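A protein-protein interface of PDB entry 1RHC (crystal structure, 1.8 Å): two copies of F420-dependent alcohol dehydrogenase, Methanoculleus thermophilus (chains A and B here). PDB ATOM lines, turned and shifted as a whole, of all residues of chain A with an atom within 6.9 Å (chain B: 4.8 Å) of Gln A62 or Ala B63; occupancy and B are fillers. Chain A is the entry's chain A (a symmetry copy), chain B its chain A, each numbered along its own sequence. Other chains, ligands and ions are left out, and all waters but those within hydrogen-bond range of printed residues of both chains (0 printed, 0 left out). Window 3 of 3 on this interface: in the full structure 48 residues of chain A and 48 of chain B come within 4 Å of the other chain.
Of the 14 printed residues of chain A, 6 touch a printed residue of chain B.
Hydrophobic or aromatic side chains of chain A that line the printed part of chain B: Ala A63, Met A95 and Tyr A96.
Of the 9 printed residues of chain B, 4 touch a printed residue of chain A.
Hydrophobic or aromatic side chains of chain B that line the printed part of chain A: Leu B20, Ala B59 and Ala B63.
Among the printed residues, 9 pairs touch across the chains.
Among the printed residues, no Asp or Glu carboxylate lies within 4 Å of a Lys or Arg side-chain nitrogen of the other chain.
OE1 of Gln A62 lies within hydrogen-bond range of OH of Tyr A96, at 2.7 Å.
Among the printed residues, pairs that only touch across the chains: Tyr A96 with Ala B59 (3.4 Å), Gly A58 with Ala B59 (3.4 Å), Ala A59 with Ala B59 (3.6 Å), Gln A62 with Ala B59 (3.7 Å), Ala A59 with Gln B62 (3.7 Å), Gln A62 with Leu B20 (3.7 Å), Ala A63 with Gln B62 (3.8 Å), Gln A62 with Ala B63 (3.8 Å) and Met A95 with Ala B59 (3.98 Å).
Ala A59 touches its own counterpart, Ala B59.
Ala A59 touches Gln B62, and with the chains exchanged Gln A62 touches Ala B59.
Gln A62 touches Ala B63, and with the chains exchanged Ala A63 touches Gln B62.
7 positions are printed for both chains.
Of the 9 pairs that touch across the chains among the printed residues, 5 have their exchanged pair printed and touching as well.
Printed residues of chain B within 4 Å of Ala A63: Gln B62.
Of the printed residues of chain B, Ala A59 touches Ala B59 and Gln B62.
Of the printed residues of chain B, Gly A58 touches Ala B59.
The nearest printed residue of chain A that does not touch Ala B63 is Ala A59 (6.8 Å).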
ATOM      1  N   TRP A  56     -19.444  22.283   7.960  1.00  0.00           N
ATOM      2  CA  TRP A  56     -19.539  22.609   9.395  1.00  0.00           C
ATOM      3  C   TRP A  56     -18.267  22.128  10.126  1.00  0.00           C
ATOM      4  O   TRP A  56     -17.740  22.814  11.014  1.00  0.00           O
ATOM      5  CB  TRP A  56     -20.768  21.921  10.004  1.00  0.00           C
ATOM      6  CG  TRP A  56     -20.972  22.251  11.476  1.00  0.00           C
ATOM      7  CD1 TRP A  56     -21.705  23.311  12.015  1.00  0.00           C
ATOM      8  CD2 TRP A  56     -20.443  21.528  12.591  1.00  0.00           C
ATOM      9  NE1 TRP A  56     -21.664  23.255  13.396  1.00  0.00           N
ATOM     10  CE2 TRP A  56     -20.901  22.177  13.774  1.00  0.00           C
ATOM     11  CE3 TRP A  56     -19.632  20.386  12.712  1.00  0.00           C
ATOM     12  CZ2 TRP A  56     -20.570  21.719  15.051  1.00  0.00           C
ATOM     13  CZ3 TRP A  56     -19.305  19.938  13.984  1.00  0.00           C
ATOM     14  CH2 TRP A  56     -19.776  20.601  15.139  1.00  0.00           C
ATOM     15  N   MET A  57     -17.769  20.945   9.755  1.00  0.00           N
ATOM     16  CA  MET A  57     -16.597  20.429  10.451  1.00  0.00           C
ATOM     17  C   MET A  57     -15.375  21.298  10.275  1.00  0.00           C
ATOM     18  O   MET A  57     -14.578  21.418  11.213  1.00  0.00           O
ATOM     19  CB  MET A  57     -16.276  18.977  10.012  1.00  0.00           C
ATOM     20  CG  MET A  57     -16.871  17.960  10.911  1.00  0.00           C
ATOM     21  SD  MET A  57     -16.270  16.272  10.475  1.00  0.00           S
ATOM     22  CE  MET A  57     -14.640  16.279  10.932  1.00  0.00           C
ATOM     23  N   GLY A  58     -15.192  21.889   9.089  1.00  0.00           N
ATOM     24  CA  GLY A  58     -14.040  22.768   8.878  1.00  0.00           C
ATOM     25  C   GLY A  58     -14.137  23.946   9.853  1.00  0.00           C
ATOM     26  O   GLY A  58     -13.161  24.366  10.496  1.00  0.00           O
ATOM     27  N   ALA A  59     -15.343  24.494   9.975  1.00  0.00           N
ATOM     28  CA  ALA A  59     -15.528  25.597  10.915  1.00  0.00           C
ATOM     29  C   ALA A  59     -15.303  25.147  12.380  1.00  0.00           C
ATOM     30  O   ALA A  59     -14.650  25.832  13.151  1.00  0.00           O
ATOM     31  CB  ALA A  59     -16.946  26.156  10.773  1.00  0.00           C
ATOM     32  N   ALA A  60     -15.820  23.982  12.754  1.00  0.00           N
ATOM     33  CA  ALA A  60     -15.705  23.523  14.158  1.00  0.00           C
ATOM     34  C   ALA A  60     -14.286  23.199  14.556  1.00  0.00           C
ATOM     35  O   ALA A  60     -13.870  23.490  15.686  1.00  0.00           O
ATOM     36  CB  ALA A  60     -16.621  22.293  14.392  1.00  0.00           C
ATOM     37  N   LEU A  61     -13.533  22.562  13.645  1.00  0.00           N
ATOM     38  CA  LEU A  61     -12.121  22.271  13.912  1.00  0.00           C
ATOM     39  C   LEU A  61     -11.331  23.574  14.089  1.00  0.00           C
ATOM     40  O   LEU A  61     -10.447  23.661  14.950  1.00  0.00           O
ATOM     41  CB  LEU A  61     -11.536  21.462  12.752  1.00  0.00           C
ATOM     42  CG  LEU A  61     -11.958  19.989  12.815  1.00  0.00           C
ATOM     43  CD1 LEU A  61     -11.797  19.372  11.415  1.00  0.00           C
ATOM     44  CD2 LEU A  61     -11.037  19.236  13.865  1.00  0.00           C
ATOM     45  N   GLN A  62     -11.638  24.579  13.271  1.00  0.00           N
ATOM     46  CA  GLN A  62     -10.946  25.846  13.357  1.00  0.00           C
ATOM     47  C   GLN A  62     -11.314  26.598  14.654  1.00  0.00           C
ATOM     48  O   GLN A  62     -10.471  27.255  15.263  1.00  0.00           O
ATOM     49  CB  GLN A  62     -11.285  26.716  12.124  1.00  0.00           C
ATOM     50  CG  GLN A  62     -10.610  28.089  12.120  1.00  0.00           C
ATOM     51  CD  GLN A  62      -9.094  28.011  12.103  1.00  0.00           C
ATOM     52  OE1 GLN A  62      -8.511  27.040  11.623  1.00  0.00           O
ATOM     53  NE2 GLN A  62      -8.447  29.065  12.586  1.00  0.00           N
ATOM     54  N   ALA A  63     -12.567  26.496  15.072  1.00  0.00           N
ATOM     55  CA  ALA A  63     -13.043  27.190  16.293  1.00  0.00           C
ATOM     56  C   ALA A  63     -12.645  26.530  17.615  1.00  0.00           C
ATOM     57  O   ALA A  63     -12.671  27.181  18.664  1.00  0.00           O
ATOM     58  CB  ALA A  63     -14.557  27.318  16.260  1.00  0.00           C
ATOM     59  N   THR A  64     -12.304  25.251  17.581  1.00  0.00           N
ATOM     60  CA  THR A  64     -11.929  24.545  18.802  1.00  0.00           C
ATOM     61  C   THR A  64     -10.421  24.348  18.924  1.00  0.00           C
ATOM     62  O   THR A  64      -9.669  24.671  18.023  1.00  0.00           O
ATOM     63  CB  THR A  64     -12.646  23.209  18.906  1.00  0.00           C
ATOM     64  OG1 THR A  64     -12.396  22.436  17.716  1.00  0.00           O
ATOM     65  CG2 THR A  64     -14.145  23.449  19.080  1.00  0.00           C
ATOM     66  N   LYS A  65      -9.970  23.804  20.043  1.00  0.00           N
ATOM     67  CA  LYS A  65      -8.544  23.701  20.245  1.00  0.00           C
ATOM     68  C   LYS A  65      -7.958  22.321  20.169  1.00  0.00           C
ATOM     69  O   LYS A  65      -6.941  22.131  19.530  1.00  0.00           O
ATOM     70  CB  LYS A  65      -8.175  24.302  21.616  1.00  0.00           C
ATOM     71  CG  LYS A  65      -8.580  25.750  21.783  1.00  0.00           C
ATOM     72  CD  LYS A  65      -8.667  26.109  23.267  1.00  0.00           C
ATOM     73  CE  LYS A  65      -9.169  27.536  23.479  1.00  0.00           C
ATOM     74  NZ  LYS A  65      -9.413  27.819  24.925  1.00  0.00           N
ATOM     75  N   ILE A  69     -12.727  15.345  16.308  1.00  0.00           N
ATOM     76  CA  ILE A  69     -14.039  15.530  15.710  1.00  0.00           C
ATOM     77  C   ILE A  69     -14.194  14.553  14.550  1.00  0.00           C
ATOM     78  O   ILE A  69     -13.267  14.344  13.765  1.00  0.00           O
ATOM     79  CB  ILE A  69     -14.218  16.997  15.210  1.00  0.00           C
ATOM     80  CG1 ILE A  69     -13.995  17.972  16.386  1.00  0.00           C
ATOM     81  CG2 ILE A  69     -15.614  17.185  14.616  1.00  0.00           C
ATOM     82  CD1 ILE A  69     -14.248  19.472  16.018  1.00  0.00           C
ATOM     83  N   MET A  95      -4.924  19.380   7.826  1.00  0.00           N
ATOM     84  CA  MET A  95      -5.039  20.708   8.452  1.00  0.00           C
ATOM     85  C   MET A  95      -5.008  20.703   9.982  1.00  0.00           C
ATOM     86  O   MET A  95      -4.447  21.619  10.594  1.00  0.00           O
ATOM     87  CB  MET A  95      -6.341  21.388   7.992  1.00  0.00           C
ATOM     88  CG  MET A  95      -6.272  21.850   6.533  1.00  0.00           C
ATOM     89  SD  MET A  95      -7.912  22.473   5.991  1.00  0.00           S
ATOM     90  CE  MET A  95      -7.897  24.066   6.694  1.00  0.00           C
ATOM     91  N   TYR A  96      -5.621  19.683  10.581  1.00  0.00           N
ATOM     92  CA  TYR A  96      -5.760  19.550  12.038  1.00  0.00           C
ATOM     93  C   TYR A  96      -5.243  18.171  12.436  1.00  0.00           C
ATOM     94  O   TYR A  96      -5.995  17.252  12.732  1.00  0.00           O
ATOM     95  CB  TYR A  96      -7.243  19.723  12.426  1.00  0.00           C
ATOM     96  CG  TYR A  96      -7.796  21.032  11.931  1.00  0.00           C
ATOM     97  CD1 TYR A  96      -8.536  21.093  10.746  1.00  0.00           C
ATOM     98  CD2 TYR A  96      -7.516  22.229  12.605  1.00  0.00           C
ATOM     99  CE1 TYR A  96      -8.973  22.312  10.240  1.00  0.00           C
ATOM    100  CE2 TYR A  96      -7.946  23.451  12.108  1.00  0.00           C
ATOM    101  CZ  TYR A  96      -8.672  23.487  10.919  1.00  0.00           C
ATOM    102  OH  TYR A  96      -9.060  24.708  10.384  1.00  0.00           O
ATOM    103  N   ARG A  99      -6.715  15.222  14.948  1.00  0.00           N
ATOM    104  CA  ARG A  99      -8.013  15.629  15.477  1.00  0.00           C
ATOM    105  C   ARG A  99      -9.200  15.236  14.615  1.00  0.00           C
ATOM    106  O   ARG A  99     -10.338  15.676  14.870  1.00  0.00           O
ATOM    107  CB  ARG A  99      -8.035  17.166  15.652  1.00  0.00           C
ATOM    108  CG  ARG A  99      -6.953  17.755  16.619  1.00  0.00           C
ATOM    109  CD  ARG A  99      -7.162  19.279  16.879  1.00  0.00           C
ATOM    110  NE  ARG A  99      -8.542  19.471  17.287  1.00  0.00           N
ATOM    111  CZ  ARG A  99      -9.274  20.562  17.055  1.00  0.00           C
ATOM    112  NH1 ARG A  99     -10.531  20.580  17.454  1.00  0.00           N
ATOM    113  NH2 ARG A  99      -8.773  21.621  16.436  1.00  0.00           N
ATOM    114  N   LEU B  20      -4.952  28.874   3.950  1.00  0.00           N
ATOM    115  CA  LEU B  20      -5.778  29.524   4.984  1.00  0.00           C
ATOM    116  C   LEU B  20      -5.044  30.753   5.527  1.00  0.00           C
ATOM    117  O   LEU B  20      -5.623  31.831   5.667  1.00  0.00           O
ATOM    118  CB  LEU B  20      -6.063  28.527   6.121  1.00  0.00           C
ATOM    119  CG  LEU B  20      -6.915  29.040   7.290  1.00  0.00           C
ATOM    120  CD1 LEU B  20      -8.200  29.630   6.782  1.00  0.00           C
ATOM    121  CD2 LEU B  20      -7.222  27.890   8.234  1.00  0.00           C
ATOM    122  N   ILE B  24      -6.176  34.809   5.403  1.00  0.00           N
ATOM    123  CA  ILE B  24      -6.229  35.709   6.553  1.00  0.00           C
ATOM    124  C   ILE B  24      -5.373  36.962   6.265  1.00  0.00           C
ATOM    125  O   ILE B  24      -5.798  38.087   6.519  1.00  0.00           O
ATOM    126  CB  ILE B  24      -5.685  34.998   7.807  1.00  0.00           C
ATOM    127  CG1 ILE B  24      -6.653  33.879   8.208  1.00  0.00           C
ATOM    128  CG2 ILE B  24      -5.491  36.023   8.954  1.00  0.00           C
ATOM    129  CD1 ILE B  24      -6.053  32.873   9.222  1.00  0.00           C
ATOM    130  N   ALA B  59     -13.499  26.269   7.423  1.00  0.00           N
ATOM    131  CA  ALA B  59     -12.406  26.770   8.253  1.00  0.00           C
ATOM    132  C   ALA B  59     -12.055  28.240   7.913  1.00  0.00           C
ATOM    133  O   ALA B  59     -11.858  29.056   8.799  1.00  0.00           O
ATOM    134  CB  ALA B  59     -11.167  25.896   8.048  1.00  0.00           C
ATOM    135  N   ALA B  60     -12.003  28.582   6.630  1.00  0.00           N
ATOM    136  CA  ALA B  60     -11.603  29.951   6.231  1.00  0.00           C
ATOM    137  C   ALA B  60     -12.613  30.999   6.632  1.00  0.00           C
ATOM    138  O   ALA B  60     -12.239  32.105   7.044  1.00  0.00           O
ATOM    139  CB  ALA B  60     -11.351  30.007   4.702  1.00  0.00           C
ATOM    140  N   LEU B  61     -13.908  30.676   6.485  1.00  0.00           N
ATOM    141  CA  LEU B  61     -14.963  31.600   6.916  1.00  0.00           C
ATOM    142  C   LEU B  61     -14.885  31.830   8.430  1.00  0.00           C
ATOM    143  O   LEU B  61     -15.084  32.954   8.906  1.00  0.00           O
ATOM    144  CB  LEU B  61     -16.332  31.023   6.547  1.00  0.00           C
ATOM    145  CG  LEU B  61     -16.641  31.202   5.055  1.00  0.00           C
ATOM    146  CD1 LEU B  61     -17.725  30.187   4.654  1.00  0.00           C
ATOM    147  CD2 LEU B  61     -17.149  32.685   4.812  1.00  0.00           C
ATOM    148  N   GLN B  62     -14.611  30.768   9.187  1.00  0.00           N
ATOM    149  CA  GLN B  62     -14.521  30.883  10.625  1.00  0.00           C
ATOM    150  C   GLN B  62     -13.273  31.688  11.046  1.00  0.00           C
ATOM    151  O   GLN B  62     -13.310  32.454  12.007  1.00  0.00           O
ATOM    152  CB  GLN B  62     -14.486  29.475  11.264  1.00  0.00           C
ATOM    153  CG  GLN B  62     -14.381  29.482  12.791  1.00  0.00           C
ATOM    154  CD  GLN B  62     -15.558  30.159  13.470  1.00  0.00           C
ATOM    155  OE1 GLN B  62     -16.663  30.207  12.931  1.00  0.00           O
ATOM    156  NE2 GLN B  62     -15.335  30.644  14.685  1.00  0.00           N
ATOM    157  N   ALA B  63     -12.174  31.514  10.324  1.00  0.00           N
ATOM    158  CA  ALA B  63     -10.910  32.217  10.644  1.00  0.00           C
ATOM    159  C   ALA B  63     -10.851  33.685  10.214  1.00  0.00           C
ATOM    160  O   ALA B  63     -10.024  34.447  10.725  1.00  0.00           O
ATOM    161  CB  ALA B  63      -9.736  31.486  10.012  1.00  0.00           C
ATOM    162  N   THR B  64     -11.692  34.078   9.270  1.00  0.00           N
ATOM    163  CA  THR B  64     -11.687  35.456   8.791  1.00  0.00           C
ATOM    164  C   THR B  64     -12.844  36.276   9.357  1.00  0.00           C
ATOM    165  O   THR B  64     -13.705  35.760  10.044  1.00  0.00           O
ATOM    166  CB  THR B  64     -11.696  35.510   7.273  1.00  0.00           C
ATOM    167  OG1 THR B  64     -12.812  34.751   6.771  1.00  0.00           O
ATOM    168  CG2 THR B  64     -10.382  34.943   6.737  1.00  0.00           C
ATOM    169  N   LYS B  65     -12.871  37.566   9.061  1.00  0.00           N
ATOM    170  CA  LYS B  65     -13.885  38.398   9.664  1.00  0.00           C
ATOM    171  C   LYS B  65     -14.975  38.886   8.756  1.00  0.00           C
ATOM    172  O   LYS B  65     -16.135  38.825   9.116  1.00  0.00           O
ATOM    173  CB  LYS B  65     -13.219  39.628  10.314  1.00  0.00           C
ATOM    174  CG  LYS B  65     -12.188  39.287  11.368  1.00  0.00           C
ATOM    175  CD  LYS B  65     -11.232  40.462  11.577  1.00  0.00           C
ATOM    176  CE  LYS B  65     -10.118  40.121  12.564  1.00  0.00           C
ATOM    177  NZ  LYS B  65      -9.098  41.209  12.631  1.00  0.00           N
